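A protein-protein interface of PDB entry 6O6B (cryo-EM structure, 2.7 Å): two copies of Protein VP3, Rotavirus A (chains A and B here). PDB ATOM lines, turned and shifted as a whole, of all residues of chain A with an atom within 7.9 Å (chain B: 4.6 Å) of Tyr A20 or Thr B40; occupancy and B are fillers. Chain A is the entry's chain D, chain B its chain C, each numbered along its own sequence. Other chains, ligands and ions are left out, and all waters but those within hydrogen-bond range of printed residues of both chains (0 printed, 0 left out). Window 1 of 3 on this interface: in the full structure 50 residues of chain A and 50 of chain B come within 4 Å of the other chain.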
ATOM      1  N   MET A   1     -22.146  15.545  20.875  1.00  0.00           N
ATOM      2  CA  MET A   1     -22.161  15.108  19.491  1.00  0.00           C
ATOM      3  C   MET A   1     -22.698  13.696  19.324  1.00  0.00           C
ATOM      4  O   MET A   1     -23.366  13.406  18.336  1.00  0.00           O
ATOM      5  CB  MET A   1     -20.776  15.166  18.913  1.00  0.00           C
ATOM      6  CG  MET A   1     -20.762  14.836  17.456  1.00  0.00           C
ATOM      7  SD  MET A   1     -19.152  14.918  16.730  1.00  0.00           S
ATOM      8  CE  MET A   1     -19.677  14.438  15.109  1.00  0.00           C
ATOM      9  N   LEU A   4     -23.426   7.417  17.365  1.00  0.00           N
ATOM     10  CA  LEU A   4     -24.054   6.128  17.626  1.00  0.00           C
ATOM     11  C   LEU A   4     -23.776   5.213  16.446  1.00  0.00           C
ATOM     12  O   LEU A   4     -24.264   5.453  15.338  1.00  0.00           O
ATOM     13  CB  LEU A   4     -25.551   6.298  17.867  1.00  0.00           C
ATOM     14  CG  LEU A   4     -25.910   7.104  19.112  1.00  0.00           C
ATOM     15  CD1 LEU A   4     -27.379   7.348  19.156  1.00  0.00           C
ATOM     16  CD2 LEU A   4     -25.475   6.408  20.366  1.00  0.00           C
ATOM     17  N   VAL A  13     -32.745   4.487   8.962  1.00  0.00           N
ATOM     18  CA  VAL A  13     -32.997   5.926   8.964  1.00  0.00           C
ATOM     19  C   VAL A  13     -34.505   6.132   8.937  1.00  0.00           C
ATOM     20  O   VAL A  13     -35.188   5.644   8.027  1.00  0.00           O
ATOM     21  CB  VAL A  13     -32.335   6.629   7.767  1.00  0.00           C
ATOM     22  CG1 VAL A  13     -32.659   8.132   7.750  1.00  0.00           C
ATOM     23  CG2 VAL A  13     -30.851   6.448   7.801  1.00  0.00           C
ATOM     24  N   ASP A  16     -36.483  11.227  11.854  1.00  0.00           N
ATOM     25  CA  ASP A  16     -35.950  11.690  13.125  1.00  0.00           C
ATOM     26  C   ASP A  16     -35.652  13.187  13.032  1.00  0.00           C
ATOM     27  O   ASP A  16     -35.777  13.801  11.970  1.00  0.00           O
ATOM     28  CB  ASP A  16     -34.709  10.878  13.471  1.00  0.00           C
ATOM     29  CG  ASP A  16     -34.364  10.923  14.950  1.00  0.00           C
ATOM     30  OD1 ASP A  16     -34.963  11.749  15.670  1.00  0.00           O
ATOM     31  OD2 ASP A  16     -33.531  10.107  15.403  1.00  0.00           O
ATOM     32  N   THR A  17     -35.227  13.789  14.149  1.00  0.00           N
ATOM     33  CA  THR A  17     -35.184  15.246  14.246  1.00  0.00           C
ATOM     34  C   THR A  17     -33.786  15.838  14.090  1.00  0.00           C
ATOM     35  O   THR A  17     -33.673  16.967  13.607  1.00  0.00           O
ATOM     36  CB  THR A  17     -35.794  15.727  15.575  1.00  0.00           C
ATOM     37  OG1 THR A  17     -35.054  15.254  16.705  1.00  0.00           O
ATOM     38  CG2 THR A  17     -37.297  15.405  15.679  1.00  0.00           C
ATOM     39  N   GLN A  18     -32.728  15.142  14.520  1.00  0.00           N
ATOM     40  CA  GLN A  18     -31.363  15.655  14.389  1.00  0.00           C
ATOM     41  C   GLN A  18     -30.370  14.601  13.931  1.00  0.00           C
ATOM     42  O   GLN A  18     -29.367  14.354  14.602  1.00  0.00           O
ATOM     43  CB  GLN A  18     -30.887  16.327  15.673  1.00  0.00           C
ATOM     44  CG  GLN A  18     -31.565  17.649  15.886  1.00  0.00           C
ATOM     45  CD  GLN A  18     -30.911  18.485  16.939  1.00  0.00           C
ATOM     46  OE1 GLN A  18     -29.846  18.146  17.443  1.00  0.00           O
ATOM     47  NE2 GLN A  18     -31.561  19.573  17.307  1.00  0.00           N
ATOM     48  N   ILE A  19     -30.626  13.971  12.791  1.00  0.00           N
ATOM     49  CA  ILE A  19     -29.869  12.810  12.343  1.00  0.00           C
ATOM     50  C   ILE A  19     -29.235  13.093  10.994  1.00  0.00           C
ATOM     51  O   ILE A  19     -29.933  13.321  10.000  1.00  0.00           O
ATOM     52  CB  ILE A  19     -30.771  11.569  12.278  1.00  0.00           C
ATOM     53  CG1 ILE A  19     -31.401  11.312  13.640  1.00  0.00           C
ATOM     54  CG2 ILE A  19     -30.012  10.345  11.830  1.00  0.00           C
ATOM     55  CD1 ILE A  19     -30.449  11.090  14.798  1.00  0.00           C
ATOM     56  N   TYR A  20     -27.911  13.053  10.965  1.00  0.00           N
ATOM     57  CA  TYR A  20     -27.159  12.822   9.748  1.00  0.00           C
ATOM     58  C   TYR A  20     -26.770  11.357   9.718  1.00  0.00           C
ATOM     59  O   TYR A  20     -26.887  10.644  10.719  1.00  0.00           O
ATOM     60  CB  TYR A  20     -25.881  13.662   9.668  1.00  0.00           C
ATOM     61  CG  TYR A  20     -26.067  15.152   9.706  1.00  0.00           C
ATOM     62  CD1 TYR A  20     -27.312  15.734   9.549  1.00  0.00           C
ATOM     63  CD2 TYR A  20     -24.985  15.981   9.915  1.00  0.00           C
ATOM     64  CE1 TYR A  20     -27.465  17.086   9.604  1.00  0.00           C
ATOM     65  CE2 TYR A  20     -25.134  17.339   9.971  1.00  0.00           C
ATOM     66  CZ  TYR A  20     -26.383  17.885   9.820  1.00  0.00           C
ATOM     67  OH  TYR A  20     -26.584  19.241   9.878  1.00  0.00           O
ATOM     68  N   THR A  21     -26.295  10.922   8.562  1.00  0.00           N
ATOM     69  CA  THR A  21     -25.728   9.600   8.404  1.00  0.00           C
ATOM     70  C   THR A  21     -24.353   9.736   7.780  1.00  0.00           C
ATOM     71  O   THR A  21     -24.098  10.636   6.978  1.00  0.00           O
ATOM     72  CB  THR A  21     -26.630   8.711   7.549  1.00  0.00           C
ATOM     73  OG1 THR A  21     -26.738   9.255   6.231  1.00  0.00           O
ATOM     74  CG2 THR A  21     -28.004   8.629   8.162  1.00  0.00           C
ATOM     75  N   HIS A  22     -23.460   8.846   8.188  1.00  0.00           N
ATOM     76  CA  HIS A  22     -22.121   8.815   7.636  1.00  0.00           C
ATOM     77  C   HIS A  22     -21.693   7.369   7.476  1.00  0.00           C
ATOM     78  O   HIS A  22     -22.018   6.522   8.310  1.00  0.00           O
ATOM     79  CB  HIS A  22     -21.134   9.561   8.525  1.00  0.00           C
ATOM     80  CG  HIS A  22     -19.754   9.604   7.965  1.00  0.00           C
ATOM     81  ND1 HIS A  22     -19.415  10.371   6.874  1.00  0.00           N
ATOM     82  CD2 HIS A  22     -18.630   8.953   8.334  1.00  0.00           C
ATOM     83  CE1 HIS A  22     -18.136  10.192   6.601  1.00  0.00           C
ATOM     84  NE2 HIS A  22     -17.636   9.338   7.472  1.00  0.00           N
ATOM     85  N   ILE A  35     -16.329  13.297  10.332  1.00  0.00           N
ATOM     86  CA  ILE A  35     -17.442  13.234  11.264  1.00  0.00           C
ATOM     87  C   ILE A  35     -17.415  14.444  12.178  1.00  0.00           C
ATOM     88  O   ILE A  35     -18.386  15.204  12.264  1.00  0.00           O
ATOM     89  CB  ILE A  35     -17.376  11.916  12.058  1.00  0.00           C
ATOM     90  CG1 ILE A  35     -17.548  10.732  11.117  1.00  0.00           C
ATOM     91  CG2 ILE A  35     -18.449  11.855  13.123  1.00  0.00           C
ATOM     92  CD1 ILE A  35     -17.144   9.443  11.702  1.00  0.00           C
ATOM     93  N   ASN A  37     -16.395  17.316  12.129  1.00  0.00           N
ATOM     94  CA  ASN A  37     -16.822  18.581  11.562  1.00  0.00           C
ATOM     95  C   ASN A  37     -18.246  18.534  11.030  1.00  0.00           C
ATOM     96  O   ASN A  37     -18.615  19.373  10.202  1.00  0.00           O
ATOM     97  CB  ASN A  37     -15.849  19.003  10.474  1.00  0.00           C
ATOM     98  CG  ASN A  37     -14.533  19.462  11.033  1.00  0.00           C
ATOM     99  OD1 ASN A  37     -14.482  20.153  12.046  1.00  0.00           O
ATOM    100  ND2 ASN A  37     -13.460  19.107  10.368  1.00  0.00           N
ATOM    101  N   LEU A  38     -19.054  17.590  11.495  1.00  0.00           N
ATOM    102  CA  LEU A  38     -20.457  17.573  11.133  1.00  0.00           C
ATOM    103  C   LEU A  38     -21.250  18.438  12.097  1.00  0.00           C
ATOM    104  O   LEU A  38     -20.892  18.607  13.264  1.00  0.00           O
ATOM    105  CB  LEU A  38     -21.002  16.147  11.123  1.00  0.00           C
ATOM    106  CG  LEU A  38     -20.439  15.224  10.037  1.00  0.00           C
ATOM    107  CD1 LEU A  38     -20.972  13.872  10.235  1.00  0.00           C
ATOM    108  CD2 LEU A  38     -20.766  15.661   8.647  1.00  0.00           C
ATOM    109  N   THR A  39     -22.344  18.989  11.583  1.00  0.00           N
ATOM    110  CA  THR A  39     -23.075  20.031  12.284  1.00  0.00           C
ATOM    111  C   THR A  39     -23.889  19.484  13.446  1.00  0.00           C
ATOM    112  O   THR A  39     -23.689  19.896  14.593  1.00  0.00           O
ATOM    113  CB  THR A  39     -23.978  20.748  11.278  1.00  0.00           C
ATOM    114  OG1 THR A  39     -23.200  21.366  10.243  1.00  0.00           O
ATOM    115  CG2 THR A  39     -25.030  21.704  11.906  1.00  0.00           C
ATOM    116  N   THR A  40     -24.797  18.560  13.173  1.00  0.00           N
ATOM    117  CA  THR A  40     -25.872  18.221  14.087  1.00  0.00           C
ATOM    118  C   THR A  40     -25.343  17.564  15.359  1.00  0.00           C
ATOM    119  O   THR A  40     -24.145  17.335  15.532  1.00  0.00           O
ATOM    120  CB  THR A  40     -26.889  17.312  13.397  1.00  0.00           C
ATOM    121  OG1 THR A  40     -28.041  17.163  14.226  1.00  0.00           O
ATOM    122  CG2 THR A  40     -26.312  15.943  13.125  1.00  0.00           C
ATOM    123  N   HIS A  41     -26.281  17.239  16.243  1.00  0.00           N
ATOM    124  CA  HIS A  41     -25.997  16.753  17.585  1.00  0.00           C
ATOM    125  C   HIS A  41     -26.055  15.237  17.700  1.00  0.00           C
ATOM    126  O   HIS A  41     -25.533  14.688  18.673  1.00  0.00           O
ATOM    127  CB  HIS A  41     -26.990  17.366  18.573  1.00  0.00           C
ATOM    128  CG  HIS A  41     -26.764  16.958  19.994  1.00  0.00           C
ATOM    129  ND1 HIS A  41     -25.691  17.400  20.737  1.00  0.00           N
ATOM    130  CD2 HIS A  41     -27.466  16.130  20.801  1.00  0.00           C
ATOM    131  CE1 HIS A  41     -25.746  16.864  21.942  1.00  0.00           C
ATOM    132  NE2 HIS A  41     -26.815  16.091  22.007  1.00  0.00           N
ATOM    133  N   ASN A  42     -26.693  14.549  16.755  1.00  0.00           N
ATOM    134  CA  ASN A  42     -26.867  13.101  16.823  1.00  0.00           C
ATOM    135  C   ASN A  42     -26.578  12.521  15.453  1.00  0.00           C
ATOM    136  O   ASN A  42     -27.192  12.928  14.462  1.00  0.00           O
ATOM    137  CB  ASN A  42     -28.270  12.728  17.277  1.00  0.00           C
ATOM    138  CG  ASN A  42     -28.582  13.247  18.645  1.00  0.00           C
ATOM    139  OD1 ASN A  42     -27.703  13.347  19.480  1.00  0.00           O
ATOM    140  ND2 ASN A  42     -29.842  13.556  18.896  1.00  0.00           N
ATOM    141  N   ILE A  43     -25.633  11.584  15.395  1.00  0.00           N
ATOM    142  CA  ILE A  43     -25.063  11.106  14.144  1.00  0.00           C
ATOM    143  C   ILE A  43     -25.125   9.591  14.156  1.00  0.00           C
ATOM    144  O   ILE A  43     -24.703   8.955  15.128  1.00  0.00           O
ATOM    145  CB  ILE A  43     -23.616  11.598  13.960  1.00  0.00           C
ATOM    146  CG1 ILE A  43     -23.580  13.135  14.125  1.00  0.00           C
ATOM    147  CG2 ILE A  43     -23.038  11.049  12.655  1.00  0.00           C
ATOM    148  CD1 ILE A  43     -22.967  14.068  13.080  1.00  0.00           C
ATOM    149  N   LEU A  44     -25.644   9.019  13.077  1.00  0.00           N
ATOM    150  CA  LEU A  44     -25.658   7.581  12.879  1.00  0.00           C
ATOM    151  C   LEU A  44     -24.492   7.214  11.975  1.00  0.00           C
ATOM    152  O   LEU A  44     -24.337   7.778  10.888  1.00  0.00           O
ATOM    153  CB  LEU A  44     -26.981   7.143  12.277  1.00  0.00           C
ATOM    154  CG  LEU A  44     -28.242   7.447  13.064  1.00  0.00           C
ATOM    155  CD1 LEU A  44     -29.429   7.101  12.219  1.00  0.00           C
ATOM    156  CD2 LEU A  44     -28.321   6.686  14.330  1.00  0.00           C
ATOM    157  N   TYR A  45     -23.683   6.273  12.429  1.00  0.00           N
ATOM    158  CA  TYR A  45     -22.449   5.881  11.765  1.00  0.00           C
ATOM    159  C   TYR A  45     -22.557   4.396  11.450  1.00  0.00           C
ATOM    160  O   TYR A  45     -22.319   3.552  12.318  1.00  0.00           O
ATOM    161  CB  TYR A  45     -21.278   6.224  12.677  1.00  0.00           C
ATOM    162  CG  TYR A  45     -19.905   5.938  12.153  1.00  0.00           C
ATOM    163  CD1 TYR A  45     -19.431   6.552  11.020  1.00  0.00           C
ATOM    164  CD2 TYR A  45     -19.043   5.131  12.854  1.00  0.00           C
ATOM    165  CE1 TYR A  45     -18.168   6.304  10.563  1.00  0.00           C
ATOM    166  CE2 TYR A  45     -17.775   4.905  12.412  1.00  0.00           C
ATOM    167  CZ  TYR A  45     -17.343   5.482  11.264  1.00  0.00           C
ATOM    168  OH  TYR A  45     -16.070   5.242  10.815  1.00  0.00           O
ATOM    169  N   PHE A  46     -22.920   4.081  10.209  1.00  0.00           N
ATOM    170  CA  PHE A  46     -23.527   2.801   9.881  1.00  0.00           C
ATOM    171  C   PHE A  46     -22.548   1.653   9.745  1.00  0.00           C
ATOM    172  O   PHE A  46     -22.866   0.553  10.206  1.00  0.00           O
ATOM    173  CB  PHE A  46     -24.335   2.910   8.582  1.00  0.00           C
ATOM    174  CG  PHE A  46     -25.644   3.653   8.701  1.00  0.00           C
ATOM    175  CD1 PHE A  46     -26.232   3.935   9.920  1.00  0.00           C
ATOM    176  CD2 PHE A  46     -26.304   4.050   7.562  1.00  0.00           C
ATOM    177  CE1 PHE A  46     -27.410   4.590   9.989  1.00  0.00           C
ATOM    178  CE2 PHE A  46     -27.497   4.717   7.643  1.00  0.00           C
ATOM    179  CZ  PHE A  46     -28.039   4.983   8.867  1.00  0.00           C
ATOM    180  N   GLN A 575     -20.892  25.290   8.875  1.00  0.00           N
ATOM    181  CA  GLN A 575     -22.198  25.902   9.080  1.00  0.00           C
ATOM    182  C   GLN A 575     -22.285  27.252   8.388  1.00  0.00           C
ATOM    183  O   GLN A 575     -23.316  27.604   7.807  1.00  0.00           O
ATOM    184  CB  GLN A 575     -22.469  26.076  10.565  1.00  0.00           C
ATOM    185  CG  GLN A 575     -22.564  24.807  11.341  1.00  0.00           C
ATOM    186  CD  GLN A 575     -22.802  25.067  12.811  1.00  0.00           C
ATOM    187  OE1 GLN A 575     -22.890  26.215  13.241  1.00  0.00           O
ATOM    188  NE2 GLN A 575     -22.891  24.006  13.592  1.00  0.00           N
ATOM    189  N   SER A 579     -24.622  27.126   4.926  1.00  0.00           N
ATOM    190  CA  SER A 579     -25.973  27.329   5.420  1.00  0.00           C
ATOM    191  C   SER A 579     -26.271  28.746   5.870  1.00  0.00           C
ATOM    192  O   SER A 579     -27.193  29.381   5.354  1.00  0.00           O
ATOM    193  CB  SER A 579     -26.212  26.394   6.595  1.00  0.00           C
ATOM    194  OG  SER A 579     -27.501  26.583   7.151  1.00  0.00           O
ATOM    195  N   THR B  17     -23.043  18.021   4.767  1.00  0.00           N
ATOM    196  CA  THR B  17     -22.852  18.802   5.986  1.00  0.00           C
ATOM    197  C   THR B  17     -24.149  19.164   6.703  1.00  0.00           C
ATOM    198  O   THR B  17     -24.129  19.298   7.929  1.00  0.00           O
ATOM    199  CB  THR B  17     -22.055  20.088   5.697  1.00  0.00           C
ATOM    200  OG1 THR B  17     -22.754  20.958   4.801  1.00  0.00           O
ATOM    201  CG2 THR B  17     -20.617  19.793   5.230  1.00  0.00           C
ATOM    202  N   GLN B  18     -25.257  19.371   5.985  1.00  0.00           N
ATOM    203  CA  GLN B  18     -26.534  19.712   6.618  1.00  0.00           C
ATOM    204  C   GLN B  18     -27.716  18.969   6.020  1.00  0.00           C
ATOM    205  O   GLN B  18     -28.680  19.590   5.567  1.00  0.00           O
ATOM    206  CB  GLN B  18     -26.780  21.218   6.615  1.00  0.00           C
ATOM    207  CG  GLN B  18     -25.890  21.922   7.594  1.00  0.00           C
ATOM    208  CD  GLN B  18     -26.308  23.332   7.863  1.00  0.00           C
ATOM    209  OE1 GLN B  18     -27.362  23.776   7.418  1.00  0.00           O
ATOM    210  NE2 GLN B  18     -25.467  24.067   8.566  1.00  0.00           N
ATOM    211  N   ILE B  19     -27.665  17.643   6.008  1.00  0.00           N
ATOM    212  CA  ILE B  19     -28.630  16.822   5.291  1.00  0.00           C
ATOM    213  C   ILE B  19     -29.334  15.885   6.254  1.00  0.00           C
ATOM    214  O   ILE B  19     -28.702  15.023   6.876  1.00  0.00           O
ATOM    215  CB  ILE B  19     -27.941  16.037   4.163  1.00  0.00           C
ATOM    216  CG1 ILE B  19     -27.237  16.998   3.217  1.00  0.00           C
ATOM    217  CG2 ILE B  19     -28.919  15.187   3.391  1.00  0.00           C
ATOM    218  CD1 ILE B  19     -28.102  18.045   2.544  1.00  0.00           C
ATOM    219  N   TYR B  20     -30.644  16.046   6.354  1.00  0.00           N
ATOM    220  CA  TYR B  20     -31.532  14.998   6.819  1.00  0.00           C
ATOM    221  C   TYR B  20     -32.143  14.338   5.598  1.00  0.00           C
ATOM    222  O   TYR B  20     -32.048  14.850   4.480  1.00  0.00           O
ATOM    223  CB  TYR B  20     -32.665  15.525   7.702  1.00  0.00           C
ATOM    224  CG  TYR B  20     -32.248  16.235   8.959  1.00  0.00           C
ATOM    225  CD1 TYR B  20     -30.948  16.181   9.427  1.00  0.00           C
ATOM    226  CD2 TYR B  20     -33.167  16.976   9.673  1.00  0.00           C
ATOM    227  CE1 TYR B  20     -30.584  16.846  10.558  1.00  0.00           C
ATOM    228  CE2 TYR B  20     -32.804  17.646  10.809  1.00  0.00           C
ATOM    229  CZ  TYR B  20     -31.506  17.579  11.244  1.00  0.00           C
ATOM    230  OH  TYR B  20     -31.092  18.241  12.372  1.00  0.00           O
ATOM    231  N   LEU B  38     -38.608  20.028  10.833  1.00  0.00           N
ATOM    232  CA  LEU B  38     -37.264  19.488  10.868  1.00  0.00           C
ATOM    233  C   LEU B  38     -36.260  20.610  11.073  1.00  0.00           C
ATOM    234  O   LEU B  38     -36.481  21.759  10.679  1.00  0.00           O
ATOM    235  CB  LEU B  38     -36.949  18.720   9.587  1.00  0.00           C
ATOM    236  CG  LEU B  38     -37.744  17.429   9.369  1.00  0.00           C
ATOM    237  CD1 LEU B  38     -37.411  16.877   8.052  1.00  0.00           C
ATOM    238  CD2 LEU B  38     -37.481  16.379  10.400  1.00  0.00           C
ATOM    239  N   THR B  39     -35.146  20.258  11.703  1.00  0.00           N
ATOM    240  CA  THR B  39     -34.203  21.245  12.197  1.00  0.00           C
ATOM    241  C   THR B  39     -33.380  21.867  11.078  1.00  0.00           C
ATOM    242  O   THR B  39     -33.408  23.088  10.892  1.00  0.00           O
ATOM    243  CB  THR B  39     -33.295  20.573  13.229  1.00  0.00           C
ATOM    244  OG1 THR B  39     -34.059  20.089  14.343  1.00  0.00           O
ATOM    245  CG2 THR B  39     -32.055  21.408  13.655  1.00  0.00           C
ATOM    246  N   THR B  40     -32.654  21.052  10.329  1.00  0.00           N
ATOM    247  CA  THR B  40     -31.566  21.517   9.489  1.00  0.00           C
ATOM    248  C   THR B  40     -32.072  22.390   8.345  1.00  0.00           C
ATOM    249  O   THR B  40     -33.270  22.617   8.170  1.00  0.00           O
ATOM    250  CB  THR B  40     -30.770  20.330   8.947  1.00  0.00           C
ATOM    251  OG1 THR B  40     -29.584  20.801   8.308  1.00  0.00           O
ATOM    252  CG2 THR B  40     -31.574  19.535   7.945  1.00  0.00           C
ATOM    253  N   HIS B  41     -31.118  22.857   7.543  1.00  0.00           N
ATOM    254  CA  HIS B  41     -31.351  23.834   6.492  1.00  0.00           C
ATOM    255  C   HIS B  41     -31.517  23.207   5.115  1.00  0.00           C
ATOM    256  O   HIS B  41     -32.026  23.870   4.209  1.00  0.00           O
ATOM    257  CB  HIS B  41     -30.189  24.828   6.449  1.00  0.00           C
ATOM    258  CG  HIS B  41     -30.345  25.900   5.419  1.00  0.00           C
ATOM    259  ND1 HIS B  41     -31.264  26.920   5.534  1.00  0.00           N
ATOM    260  CD2 HIS B  41     -29.709  26.099   4.241  1.00  0.00           C
ATOM    261  CE1 HIS B  41     -31.182  27.703   4.474  1.00  0.00           C
ATOM    262  NE2 HIS B  41     -30.245  27.228   3.676  1.00  0.00           N
ATOM    263  N   ASN B  42     -31.083  21.962   4.924  1.00  0.00           N
ATOM    264  CA  ASN B  42     -31.129  21.309   3.619  1.00  0.00           C
ATOM    265  C   ASN B  42     -31.628  19.890   3.814  1.00  0.00           C
ATOM    266  O   ASN B  42     -31.052  19.129   4.598  1.00  0.00           O
ATOM    267  CB  ASN B  42     -29.765  21.309   2.945  1.00  0.00           C
ATOM    268  CG  ASN B  42     -29.253  22.690   2.697  1.00  0.00           C
ATOM    269  OD1 ASN B  42     -30.027  23.599   2.455  1.00  0.00           O
ATOM    270  ND2 ASN B  42     -27.944  22.860   2.728  1.00  0.00           N
ATOM    271  N   ILE B  43     -32.708  19.543   3.116  1.00  0.00           N
ATOM    272  CA  ILE B  43     -33.457  18.320   3.367  1.00  0.00           C
ATOM    273  C   ILE B  43     -33.629  17.603   2.041  1.00  0.00           C
ATOM    274  O   ILE B  43     -34.054  18.210   1.052  1.00  0.00           O
ATOM    275  CB  ILE B  43     -34.822  18.618   4.014  1.00  0.00           C
ATOM    276  CG1 ILE B  43     -34.603  19.495   5.269  1.00  0.00           C
ATOM    277  CG2 ILE B  43     -35.595  17.316   4.232  1.00  0.00           C
ATOM    278  CD1 ILE B  43     -35.158  19.126   6.647  1.00  0.00           C
ATOM    279  N   ARG B 571     -40.687  23.621  15.069  1.00  0.00           N
ATOM    280  CA  ARG B 571     -39.311  23.437  14.630  1.00  0.00           C
ATOM    281  C   ARG B 571     -38.322  23.720  15.750  1.00  0.00           C
ATOM    282  O   ARG B 571     -37.357  22.971  15.939  1.00  0.00           O
ATOM    283  CB  ARG B 571     -39.034  24.336  13.433  1.00  0.00           C
ATOM    284  CG  ARG B 571     -37.686  24.159  12.816  1.00  0.00           C
ATOM    285  CD  ARG B 571     -37.489  25.100  11.661  1.00  0.00           C
ATOM    286  NE  ARG B 571     -38.399  24.794  10.577  1.00  0.00           N
ATOM    287  CZ  ARG B 571     -38.094  24.104   9.483  1.00  0.00           C
ATOM    288  NH1 ARG B 571     -36.897  23.550   9.290  1.00  0.00           N
ATOM    289  NH2 ARG B 571     -39.040  23.911   8.584  1.00  0.00           N
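O of Thr A17 sits at hydrogen-bond distance from OG1 of Thr B39 (3.2 Å).
The backbone carbonyl oxygen of Thr B17 lies close to the side-chain hydroxyl of Tyr A20.
The side-chain amide oxygen of Gln B18 is in hydrogen-bond range of the side-chain hydroxyl of Ser A579 (2.8 Å).
OH of Tyr B20 sits close to O of Thr A17 (3.1 Å).
The backbone carbonyl oxygen (O) of Thr B17 sits at hydrogen-bond distance from the side-chain hydroxyl (OG1) of Thr A39.
The backbone NH of Asn A42 sits close to the backbone carbonyl oxygen of Gln A18 (3.4 Å).
The side-chain hydroxyl of Thr A40 lies within hydrogen-bond range of the backbone carbonyl oxygen of Gln A18 (3.1 Å).
The backbone carbonyl oxygen (O) of Gln B18 lies close to the backbone NH (N) of Asn B42, 3.4 Å away.
O of Tyr A20 lies within hydrogen-bond range of N of Leu A44 (3.1 Å).
The side-chain hydroxyl of Thr B40 is in hydrogen-bond range of the backbone carbonyl oxygen of Gln B18 (3.1 Å).
Among the printed residues, merely in contact across the chains: Asp A16 with Leu B38 (3.5 Å), Gln A18 with Tyr B20 (3.3 Å), Gln A18 with Thr B39 (3.8 Å), Ile A19 with Ile B19 (3.8 Å), Ile A19 with Tyr B20 (3.1 Å), Tyr A20 with Gln B18 (3.3 Å), Tyr A20 with Ile B19 (3.1 Å), Tyr A20 with Tyr B20 (3.3 Å), Tyr A20 with Thr B40 (3.7 Å), Thr A39 with Gln B18 (3.8 Å), Thr A40 with Tyr B20 (3.7 Å), Gln A575 with Gln B18 (3.8 Å) and Ser A579 with His B41 (3.3 Å).
Of the printed residues of chain B, Ile A19 touches Ile B19 and Tyr B20.
Tyr A20 touches five residues of chain B.
Leu A38 touches none of the printed residues of chain B.
Printed residues of chain B within 4 Å of Gln A575: Gln B18.
Of the printed residues of chain A, Thr B17 touches Tyr A20 (3.0 Å) and Thr A39 (3.2 Å).
Of the printed residues of chain A, Leu B38 touches Asp A16.
Of the printed residues of chain A, His B41 touches Ser A579 (3.3 Å).
Ile B43 touches none of the printed residues of chain A.
The nearest printed residue of chain B that does not touch Tyr A20 is His B41 (6.3 Å).
Of the 23 printed residues of chain A, 9 touch a printed residue of chain B.
Hydrophobic or aromatic side chains of chain B that line the printed part of chain A: Tyr B20, Leu B38 and His B41.
Among the printed residues, 18 pairs touch across the chains.
Among the printed residues, no Asp or Glu carboxylate lies within 4 Å of a Lys or Arg side-chain nitrogen of the other chain.
Thr A17 touches Tyr B20, and with the chains exchanged Tyr A20 touches Thr B17.
Thr A17 touches Thr B39, and with the chains exchanged Thr A39 touches Thr B17.
Gln A18 touches Tyr B20, and with the chains exchanged Tyr A20 touches Gln B18.
Tyr A20 touches Thr B40, and with the chains exchanged Thr A40 touches Tyr B20.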
